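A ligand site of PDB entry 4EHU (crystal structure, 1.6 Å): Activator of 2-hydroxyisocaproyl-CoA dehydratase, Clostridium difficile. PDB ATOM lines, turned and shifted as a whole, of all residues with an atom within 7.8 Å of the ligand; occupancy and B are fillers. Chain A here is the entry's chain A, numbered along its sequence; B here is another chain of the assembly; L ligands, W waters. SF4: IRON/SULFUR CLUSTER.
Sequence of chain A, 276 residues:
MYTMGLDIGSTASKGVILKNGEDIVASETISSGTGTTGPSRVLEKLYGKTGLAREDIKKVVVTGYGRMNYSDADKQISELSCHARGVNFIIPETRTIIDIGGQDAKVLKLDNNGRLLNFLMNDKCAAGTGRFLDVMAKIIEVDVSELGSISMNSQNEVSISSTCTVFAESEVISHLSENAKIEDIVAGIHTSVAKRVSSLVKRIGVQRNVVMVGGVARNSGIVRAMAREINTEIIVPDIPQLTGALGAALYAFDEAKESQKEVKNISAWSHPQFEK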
ATOM      1  N   LYS A 124      -0.458 -17.121   2.676  1.00  0.00           N
ATOM      2  CA  LYS A 124      -0.315 -18.256   1.762  1.00  0.00           C
ATOM      3  C   LYS A 124       0.815 -19.168   2.186  1.00  0.00           C
ATOM      4  O   LYS A 124       1.044 -20.197   1.555  1.00  0.00           O
ATOM      5  CB  LYS A 124      -0.113 -17.776   0.333  1.00  0.00           C
ATOM      6  CG  LYS A 124      -1.241 -16.910  -0.173  1.00  0.00           C
ATOM      7  CD  LYS A 124      -2.588 -17.545   0.111  1.00  0.00           C
ATOM      8  CE  LYS A 124      -3.697 -16.875  -0.681  1.00  0.00           C
ATOM      9  NZ  LYS A 124      -5.040 -17.248  -0.169  1.00  0.00           N
ATOM     10  N   CYS A 125       1.513 -18.778   3.242  1.00  0.00           N
ATOM     11  CA  CYS A 125       2.834 -19.338   3.548  1.00  0.00           C
ATOM     12  C   CYS A 125       2.890 -19.723   5.019  1.00  0.00           C
ATOM     13  O   CYS A 125       2.507 -18.924   5.882  1.00  0.00           O
ATOM     14  CB  CYS A 125       3.909 -18.277   3.267  1.00  0.00           C
ATOM     15  SG  CYS A 125       5.575 -18.645   3.852  1.00  0.00           S
ATOM     16  N   ALA A 126       3.327 -20.938   5.330  1.00  0.00           N
ATOM     17  CA  ALA A 126       3.361 -21.362   6.737  1.00  0.00           C
ATOM     18  C   ALA A 126       4.404 -20.593   7.569  1.00  0.00           C
ATOM     19  O   ALA A 126       4.276 -20.517   8.821  1.00  0.00           O
ATOM     20  CB  ALA A 126       3.617 -22.841   6.824  1.00  0.00           C
ATOM     21  N   ALA A 127       5.432 -20.049   6.918  1.00  0.00           N
ATOM     22  CA  ALA A 127       6.465 -19.356   7.668  1.00  0.00           C
ATOM     23  C   ALA A 127       5.824 -18.125   8.313  1.00  0.00           C
ATOM     24  O   ALA A 127       4.885 -17.543   7.756  1.00  0.00           O
ATOM     25  CB  ALA A 127       7.607 -18.933   6.734  1.00  0.00           C
ATOM     26  N   GLY A 128       6.354 -17.704   9.442  1.00  0.00           N
ATOM     27  CA  GLY A 128       5.876 -16.489  10.091  1.00  0.00           C
ATOM     28  C   GLY A 128       4.483 -16.653  10.656  1.00  0.00           C
ATOM     29  O   GLY A 128       3.776 -15.665  10.847  1.00  0.00           O
ATOM     30  N   PHE A 132       4.555 -22.593  11.684  1.00  0.00           N
ATOM     31  CA  PHE A 132       6.006 -22.695  11.673  1.00  0.00           C
ATOM     32  C   PHE A 132       6.487 -23.133  13.067  1.00  0.00           C
ATOM     33  O   PHE A 132       7.306 -24.036  13.209  1.00  0.00           O
ATOM     34  CB  PHE A 132       6.611 -21.344  11.260  1.00  0.00           C
ATOM     35  CG  PHE A 132       8.142 -21.283  11.239  1.00  0.00           C
ATOM     36  CD1 PHE A 132       8.831 -21.499  10.059  1.00  0.00           C
ATOM     37  CD2 PHE A 132       8.861 -20.937  12.385  1.00  0.00           C
ATOM     38  CE1 PHE A 132      10.221 -21.412  10.005  1.00  0.00           C
ATOM     39  CE2 PHE A 132      10.241 -20.836  12.345  1.00  0.00           C
ATOM     40  CZ  PHE A 132      10.935 -21.074  11.148  1.00  0.00           C
ATOM     41  N   THR A 163      14.079 -18.845   4.917  1.00  0.00           N
ATOM     42  CA  THR A 163      12.846 -18.254   5.392  1.00  0.00           C
ATOM     43  C   THR A 163      11.672 -19.237   5.234  1.00  0.00           C
ATOM     44  O   THR A 163      10.646 -19.040   5.872  1.00  0.00           O
ATOM     45  CB  THR A 163      12.498 -16.966   4.603  1.00  0.00           C
ATOM     46  OG1 THR A 163      12.601 -17.209   3.206  1.00  0.00           O
ATOM     47  CG2 THR A 163      13.440 -15.839   4.972  1.00  0.00           C
ATOM     48  N   CYS A 164      11.858 -20.297   4.450  1.00  0.00           N
ATOM     49  CA  CYS A 164      10.816 -21.300   4.219  1.00  0.00           C
ATOM     50  C   CYS A 164      10.750 -22.260   5.408  1.00  0.00           C
ATOM     51  O   CYS A 164      11.792 -22.694   5.922  1.00  0.00           O
ATOM     52  CB  CYS A 164      11.154 -22.062   2.944  1.00  0.00           C
ATOM     53  SG  CYS A 164      10.177 -23.571   2.641  1.00  0.00           S
ATOM     54  N   THR A 165       9.542 -22.596   5.855  1.00  0.00           N
ATOM     55  CA  THR A 165       9.371 -23.564   6.934  1.00  0.00           C
ATOM     56  C   THR A 165      10.093 -24.885   6.652  1.00  0.00           C
ATOM     57  O   THR A 165      10.746 -25.453   7.541  1.00  0.00           O
ATOM     58  CB  THR A 165       7.877 -23.864   7.155  1.00  0.00           C
ATOM     59  OG1 THR A 165       7.159 -22.652   7.391  1.00  0.00           O
ATOM     60  CG2 THR A 165       7.691 -24.828   8.320  1.00  0.00           C
ATOM     61  N   VAL A 166       9.952 -25.379   5.425  1.00  0.00           N
ATOM     62  CA  VAL A 166      10.492 -26.695   5.064  1.00  0.00           C
ATOM     63  C   VAL A 166      12.011 -26.672   5.101  1.00  0.00           C
ATOM     64  O   VAL A 166      12.635 -27.535   5.689  1.00  0.00           O
ATOM     65  CB  VAL A 166       9.997 -27.139   3.689  1.00  0.00           C
ATOM     66  CG1 VAL A 166      10.572 -28.517   3.375  1.00  0.00           C
ATOM     67  CG2 VAL A 166       8.463 -27.157   3.700  1.00  0.00           C
ATOM     68  N   PHE A 167      12.614 -25.675   4.438  1.00  0.00           N
ATOM     69  CA  PHE A 167      14.069 -25.565   4.446  1.00  0.00           C
ATOM     70  C   PHE A 167      14.603 -25.243   5.852  1.00  0.00           C
ATOM     71  O   PHE A 167      15.680 -25.716   6.237  1.00  0.00           O
ATOM     72  CB  PHE A 167      14.544 -24.528   3.435  1.00  0.00           C
ATOM     73  CG  PHE A 167      14.267 -24.902   2.003  1.00  0.00           C
ATOM     74  CD1 PHE A 167      14.408 -26.213   1.564  1.00  0.00           C
ATOM     75  CD2 PHE A 167      13.869 -23.935   1.097  1.00  0.00           C
ATOM     76  CE1 PHE A 167      14.163 -26.559   0.237  1.00  0.00           C
ATOM     77  CE2 PHE A 167      13.604 -24.276  -0.243  1.00  0.00           C
ATOM     78  CZ  PHE A 167      13.765 -25.591  -0.669  1.00  0.00           C
ATOM     79  N   ALA A 168      13.865 -24.445   6.611  1.00  0.00           N
ATOM     80  CA  ALA A 168      14.301 -24.080   7.963  1.00  0.00           C
ATOM     81  C   ALA A 168      14.294 -25.320   8.858  1.00  0.00           C
ATOM     82  O   ALA A 168      15.158 -25.480   9.718  1.00  0.00           O
ATOM     83  CB  ALA A 168      13.388 -22.992   8.554  1.00  0.00           C
ATOM     84  N   ARG A 196       9.864 -12.238   9.686  1.00  0.00           N
ATOM     85  CA  ARG A 196       8.850 -12.300   8.641  1.00  0.00           C
ATOM     86  C   ARG A 196       7.630 -11.425   8.946  1.00  0.00           C
ATOM     87  O   ARG A 196       7.074 -10.800   8.036  1.00  0.00           O
ATOM     88  CB  ARG A 196       8.428 -13.747   8.401  1.00  0.00           C
ATOM     89  CG  ARG A 196       7.374 -13.868   7.349  1.00  0.00           C
ATOM     90  CD  ARG A 196       7.314 -15.274   6.802  1.00  0.00           C
ATOM     91  NE  ARG A 196       6.097 -15.411   6.019  1.00  0.00           N
ATOM     92  CZ  ARG A 196       5.963 -14.939   4.791  1.00  0.00           C
ATOM     93  NH1 ARG A 196       6.966 -14.302   4.198  1.00  0.00           N
ATOM     94  NH2 ARG A 196       4.809 -15.087   4.138  1.00  0.00           N
ATOM     95  N   ASN B 122      13.599 -19.626  -8.364  1.00  0.00           N
ATOM     96  CA  ASN B 122      12.959 -19.718  -7.058  1.00  0.00           C
ATOM     97  C   ASN B 122      13.858 -20.548  -6.170  1.00  0.00           C
ATOM     98  O   ASN B 122      13.943 -21.764  -6.358  1.00  0.00           O
ATOM     99  CB  ASN B 122      11.591 -20.402  -7.089  1.00  0.00           C
ATOM    100  CG  ASN B 122      11.219 -20.961  -5.695  1.00  0.00           C
ATOM    101  OD1 ASN B 122      11.536 -20.342  -4.686  1.00  0.00           O
ATOM    102  ND2 ASN B 122      10.599 -22.153  -5.643  1.00  0.00           N
ATOM    103  N   LYS B 124      13.837 -19.804  -2.649  1.00  0.00           N
ATOM    104  CA  LYS B 124      13.438 -19.454  -1.276  1.00  0.00           C
ATOM    105  C   LYS B 124      12.242 -20.228  -0.757  1.00  0.00           C
ATOM    106  O   LYS B 124      11.987 -20.214   0.438  1.00  0.00           O
ATOM    107  CB  LYS B 124      13.166 -17.957  -1.141  1.00  0.00           C
ATOM    108  CG  LYS B 124      14.445 -17.114  -1.159  1.00  0.00           C
ATOM    109  CD  LYS B 124      15.518 -17.617  -0.181  1.00  0.00           C
ATOM    110  CE  LYS B 124      15.109 -17.429   1.284  1.00  0.00           C
ATOM    111  NZ  LYS B 124      16.235 -17.741   2.218  1.00  0.00           N
ATOM    112  N   CYS B 125      11.504 -20.881  -1.656  1.00  0.00           N
ATOM    113  CA  CYS B 125      10.277 -21.588  -1.309  1.00  0.00           C
ATOM    114  C   CYS B 125      10.365 -23.038  -1.749  1.00  0.00           C
ATOM    115  O   CYS B 125      10.706 -23.318  -2.898  1.00  0.00           O
ATOM    116  CB  CYS B 125       9.082 -20.894  -1.981  1.00  0.00           C
ATOM    117  SG  CYS B 125       7.515 -21.748  -1.875  1.00  0.00           S
ATOM    118  N   ALA B 126      10.067 -23.983  -0.863  1.00  0.00           N
ATOM    119  CA  ALA B 126      10.166 -25.387  -1.240  1.00  0.00           C
ATOM    120  C   ALA B 126       9.104 -25.798  -2.256  1.00  0.00           C
ATOM    121  O   ALA B 126       9.271 -26.818  -2.943  1.00  0.00           O
ATOM    122  CB  ALA B 126      10.071 -26.272  -0.041  1.00  0.00           C
ATOM    123  N   ALA B 127       8.003 -25.064  -2.324  1.00  0.00           N
ATOM    124  CA  ALA B 127       6.966 -25.404  -3.306  1.00  0.00           C
ATOM    125  C   ALA B 127       7.535 -25.202  -4.700  1.00  0.00           C
ATOM    126  O   ALA B 127       8.383 -24.337  -4.925  1.00  0.00           O
ATOM    127  CB  ALA B 127       5.717 -24.526  -3.099  1.00  0.00           C
ATOM    128  N   GLY B 128       7.062 -25.971  -5.668  1.00  0.00           N
ATOM    129  CA  GLY B 128       7.567 -25.826  -7.030  1.00  0.00           C
ATOM    130  C   GLY B 128       9.011 -26.261  -7.199  1.00  0.00           C
ATOM    131  O   GLY B 128       9.692 -25.853  -8.144  1.00  0.00           O
ATOM    132  N   PHE B 132       9.194 -30.403  -2.703  1.00  0.00           N
ATOM    133  CA  PHE B 132       7.739 -30.536  -2.572  1.00  0.00           C
ATOM    134  C   PHE B 132       7.328 -31.976  -2.889  1.00  0.00           C
ATOM    135  O   PHE B 132       6.567 -32.609  -2.138  1.00  0.00           O
ATOM    136  CB  PHE B 132       7.055 -29.574  -3.553  1.00  0.00           C
ATOM    137  CG  PHE B 132       5.544 -29.541  -3.482  1.00  0.00           C
ATOM    138  CD1 PHE B 132       4.885 -28.633  -2.651  1.00  0.00           C
ATOM    139  CD2 PHE B 132       4.788 -30.352  -4.321  1.00  0.00           C
ATOM    140  CE1 PHE B 132       3.482 -28.581  -2.618  1.00  0.00           C
ATOM    141  CE2 PHE B 132       3.410 -30.296  -4.309  1.00  0.00           C
ATOM    142  CZ  PHE B 132       2.736 -29.406  -3.471  1.00  0.00           C
ATOM    143  N   THR B 163      -0.780 -23.462  -1.938  1.00  0.00           N
ATOM    144  CA  THR B 163       0.439 -23.391  -2.736  1.00  0.00           C
ATOM    145  C   THR B 163       1.667 -23.705  -1.876  1.00  0.00           C
ATOM    146  O   THR B 163       2.709 -24.060  -2.405  1.00  0.00           O
ATOM    147  CB  THR B 163       0.598 -22.023  -3.429  1.00  0.00           C
ATOM    148  OG1 THR B 163       0.413 -20.974  -2.474  1.00  0.00           O
ATOM    149  CG2 THR B 163      -0.433 -21.866  -4.544  1.00  0.00           C
ATOM    150  N   CYS B 164       1.505 -23.645  -0.555  1.00  0.00           N
ATOM    151  CA  CYS B 164       2.622 -23.886   0.365  1.00  0.00           C
ATOM    152  C   CYS B 164       2.824 -25.391   0.588  1.00  0.00           C
ATOM    153  O   CYS B 164       1.843 -26.119   0.732  1.00  0.00           O
ATOM    154  CB  CYS B 164       2.302 -23.192   1.665  1.00  0.00           C
ATOM    155  SG  CYS B 164       3.365 -23.650   3.096  1.00  0.00           S
ATOM    156  N   THR B 165       4.070 -25.854   0.608  1.00  0.00           N
ATOM    157  CA  THR B 165       4.351 -27.272   0.862  1.00  0.00           C
ATOM    158  C   THR B 165       3.726 -27.780   2.176  1.00  0.00           C
ATOM    159  O   THR B 165       3.201 -28.891   2.248  1.00  0.00           O
ATOM    160  CB  THR B 165       5.882 -27.512   0.930  1.00  0.00           C
ATOM    161  OG1 THR B 165       6.499 -27.017  -0.261  1.00  0.00           O
ATOM    162  CG2 THR B 165       6.217 -28.987   1.110  1.00  0.00           C
ATOM    163  N   VAL B 166       3.827 -26.968   3.230  1.00  0.00           N
ATOM    164  CA  VAL B 166       3.356 -27.378   4.548  1.00  0.00           C
ATOM    165  C   VAL B 166       1.836 -27.490   4.557  1.00  0.00           C
ATOM    166  O   VAL B 166       1.299 -28.491   4.970  1.00  0.00           O
ATOM    167  CB  VAL B 166       3.816 -26.381   5.629  1.00  0.00           C
ATOM    168  CG1 VAL B 166       3.358 -26.831   7.005  1.00  0.00           C
ATOM    169  CG2 VAL B 166       5.347 -26.245   5.567  1.00  0.00           C
ATOM    170  N   PHE B 167       1.166 -26.462   4.069  1.00  0.00           N
ATOM    171  CA  PHE B 167      -0.292 -26.486   4.029  1.00  0.00           C
ATOM    172  C   PHE B 167      -0.769 -27.573   3.026  1.00  0.00           C
ATOM    173  O   PHE B 167      -1.798 -28.230   3.263  1.00  0.00           O
ATOM    174  CB  PHE B 167      -0.842 -25.103   3.648  1.00  0.00           C
ATOM    175  CG  PHE B 167      -0.626 -24.047   4.714  1.00  0.00           C
ATOM    176  CD1 PHE B 167      -0.659 -24.371   6.062  1.00  0.00           C
ATOM    177  CD2 PHE B 167      -0.390 -22.732   4.359  1.00  0.00           C
ATOM    178  CE1 PHE B 167      -0.465 -23.391   7.065  1.00  0.00           C
ATOM    179  CE2 PHE B 167      -0.200 -21.740   5.333  1.00  0.00           C
ATOM    180  CZ  PHE B 167      -0.234 -22.077   6.686  1.00  0.00           C
ATOM    181  N   ALA B 168      -0.021 -27.787   1.947  1.00  0.00           N
ATOM    182  CA  ALA B 168      -0.419 -28.786   0.937  1.00  0.00           C
ATOM    183  C   ALA B 168      -0.299 -30.184   1.533  1.00  0.00           C
ATOM    184  O   ALA B 168      -1.114 -31.065   1.286  1.00  0.00           O
ATOM    185  CB  ALA B 168       0.445 -28.643  -0.351  1.00  0.00           C
ATOM    186  N   ARG B 196       3.261 -23.543 -10.164  1.00  0.00           N
ATOM    187  CA  ARG B 196       4.255 -22.669  -9.548  1.00  0.00           C
ATOM    188  C   ARG B 196       5.486 -22.411 -10.449  1.00  0.00           C
ATOM    189  O   ARG B 196       5.962 -21.295 -10.520  1.00  0.00           O
ATOM    190  CB  ARG B 196       4.692 -23.205  -8.183  1.00  0.00           C
ATOM    191  CG  ARG B 196       5.660 -22.282  -7.485  1.00  0.00           C
ATOM    192  CD  ARG B 196       5.983 -22.703  -6.071  1.00  0.00           C
ATOM    193  NE  ARG B 196       7.172 -22.015  -5.587  1.00  0.00           N
ATOM    194  CZ  ARG B 196       7.230 -20.707  -5.355  1.00  0.00           C
ATOM    195  NH1 ARG B 196       6.159 -19.952  -5.538  1.00  0.00           N
ATOM    196  NH2 ARG B 196       8.361 -20.158  -4.932  1.00  0.00           N
HETATM  197 FE1  SF4 L   1       8.034 -22.633   2.472  1.00  0.00          FE
HETATM  198 FE2  SF4 L   1       5.414 -22.898   2.346  1.00  0.00          FE
HETATM  199 FE3  SF4 L   1       6.866 -21.830   0.305  1.00  0.00          FE
HETATM  200 FE4  SF4 L   1       6.370 -20.491   2.719  1.00  0.00          FE
HETATM  201  S1  SF4 L   1       4.956 -21.126   1.140  1.00  0.00           S
HETATM  202  S2  SF4 L   1       8.272 -20.670   1.625  1.00  0.00           S
HETATM  203  S3  SF4 L   1       6.586 -22.210   4.135  1.00  0.00           S
HETATM  204  S4  SF4 L   1       6.886 -23.898   0.993  1.00  0.00           S
HETATM  205  O   HOH W   1       2.619 -19.769  -0.950  1.00  0.00           O
HETATM  206  O   HOH W   2      10.428 -17.931   1.578  1.00  0.00           O
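Water W1 lies within hydrogen-bond range of the side-chain hydroxyl (OG1) of Thr 163 of chain B (2.9 Å), the backbone carbonyl oxygen (O) of Lys 124 of chain A (3.0 Å) and a sulfur (S1) of the ligand (3.4 Å).
Water W2 lies within hydrogen-bond range of the side-chain hydroxyl (OG1) of Thr 163 of chain A (2.8 Å), the backbone carbonyl oxygen (O) of Lys 124 of chain B (3.0 Å) and a sulfur (S2) of the ligand (3.5 Å).
The backbone NH (N) of Ala 126 of chain A sits close to the side-chain sulfur (SG) of Cys 164 of chain B (3.5 Å).
The side-chain sulfur (SG) of Cys 164 of chain B lies close to the backbone NH (N) of Phe 167 of chain B, at 3.7 Å.
The backbone NH (N) of Ala 127 of chain B lies close to the side-chain sulfur (SG) of Cys 125 of chain B (3.4 Å).
The side-chain sulfur of Cys 164 of chain A lies close to the backbone NH of Phe 167 of chain A (3.7 Å).
The backbone NH of Lys 124 of chain B lies within hydrogen-bond range of the side-chain amide oxygen of Asn 122 of chain B, at 3.1 Å.
The backbone NH (N) of Ala 127 of chain A is in hydrogen-bond range of the side-chain hydroxyl (OG1) of Thr 165 of chain A.
The guanidinium group (NE) of Arg 196 of chain A sits at hydrogen-bond distance from the backbone carbonyl oxygen (O) of Ala 127 of chain A, 3.0 Å away.
The side-chain hydroxyl (OG1) of Thr 165 of chain B lies within hydrogen-bond range of the backbone NH (N) of Ala 127 of chain B (3.2 Å).
Residues that only touch the ligand: Lys 124 of chain B (3.9 Å).
N of Ala 127 of chain A sits close to S3 of the ligand (3.7 Å).
N of Thr 165 of chain A lies close to S3 of the ligand (3.4 Å).
The side-chain hydroxyl (OG1) of Thr 165 of chain A lies close to a sulfur (S3) of the ligand, 3.3 Å away.
S4 of the ligand lies close to OG1 of Thr 165 of chain B (3.4 Å).
N of Thr 165 of chain B lies close to S4 of the ligand (3.5 Å).
The side-chain sulfur (SG) of Cys 164 of chain B binds an iron atom (FE2) of the ligand, 2.3 Å away.
An iron atom (FE1) of the ligand is bound by the side-chain sulfur (SG) of Cys 164 of chain A.
A sulfur (S4) of the ligand lies close to the backbone NH (N) of Ala 127 of chain B, 3.7 Å away.
The side-chain sulfur (SG) of Cys 125 of chain B binds an iron atom (FE3) of the ligand (2.3 Å).
A sulfur (S4) of the ligand sits close to the backbone NH (N) of Ala 126 of chain B.
An iron atom (FE4) of the ligand is bound by the side-chain sulfur (SG) of Cys 125 of chain A, 2.3 Å away.
A sulfur (S3) of the ligand sits close to the backbone NH (N) of Ala 126 of chain A (3.7 Å).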
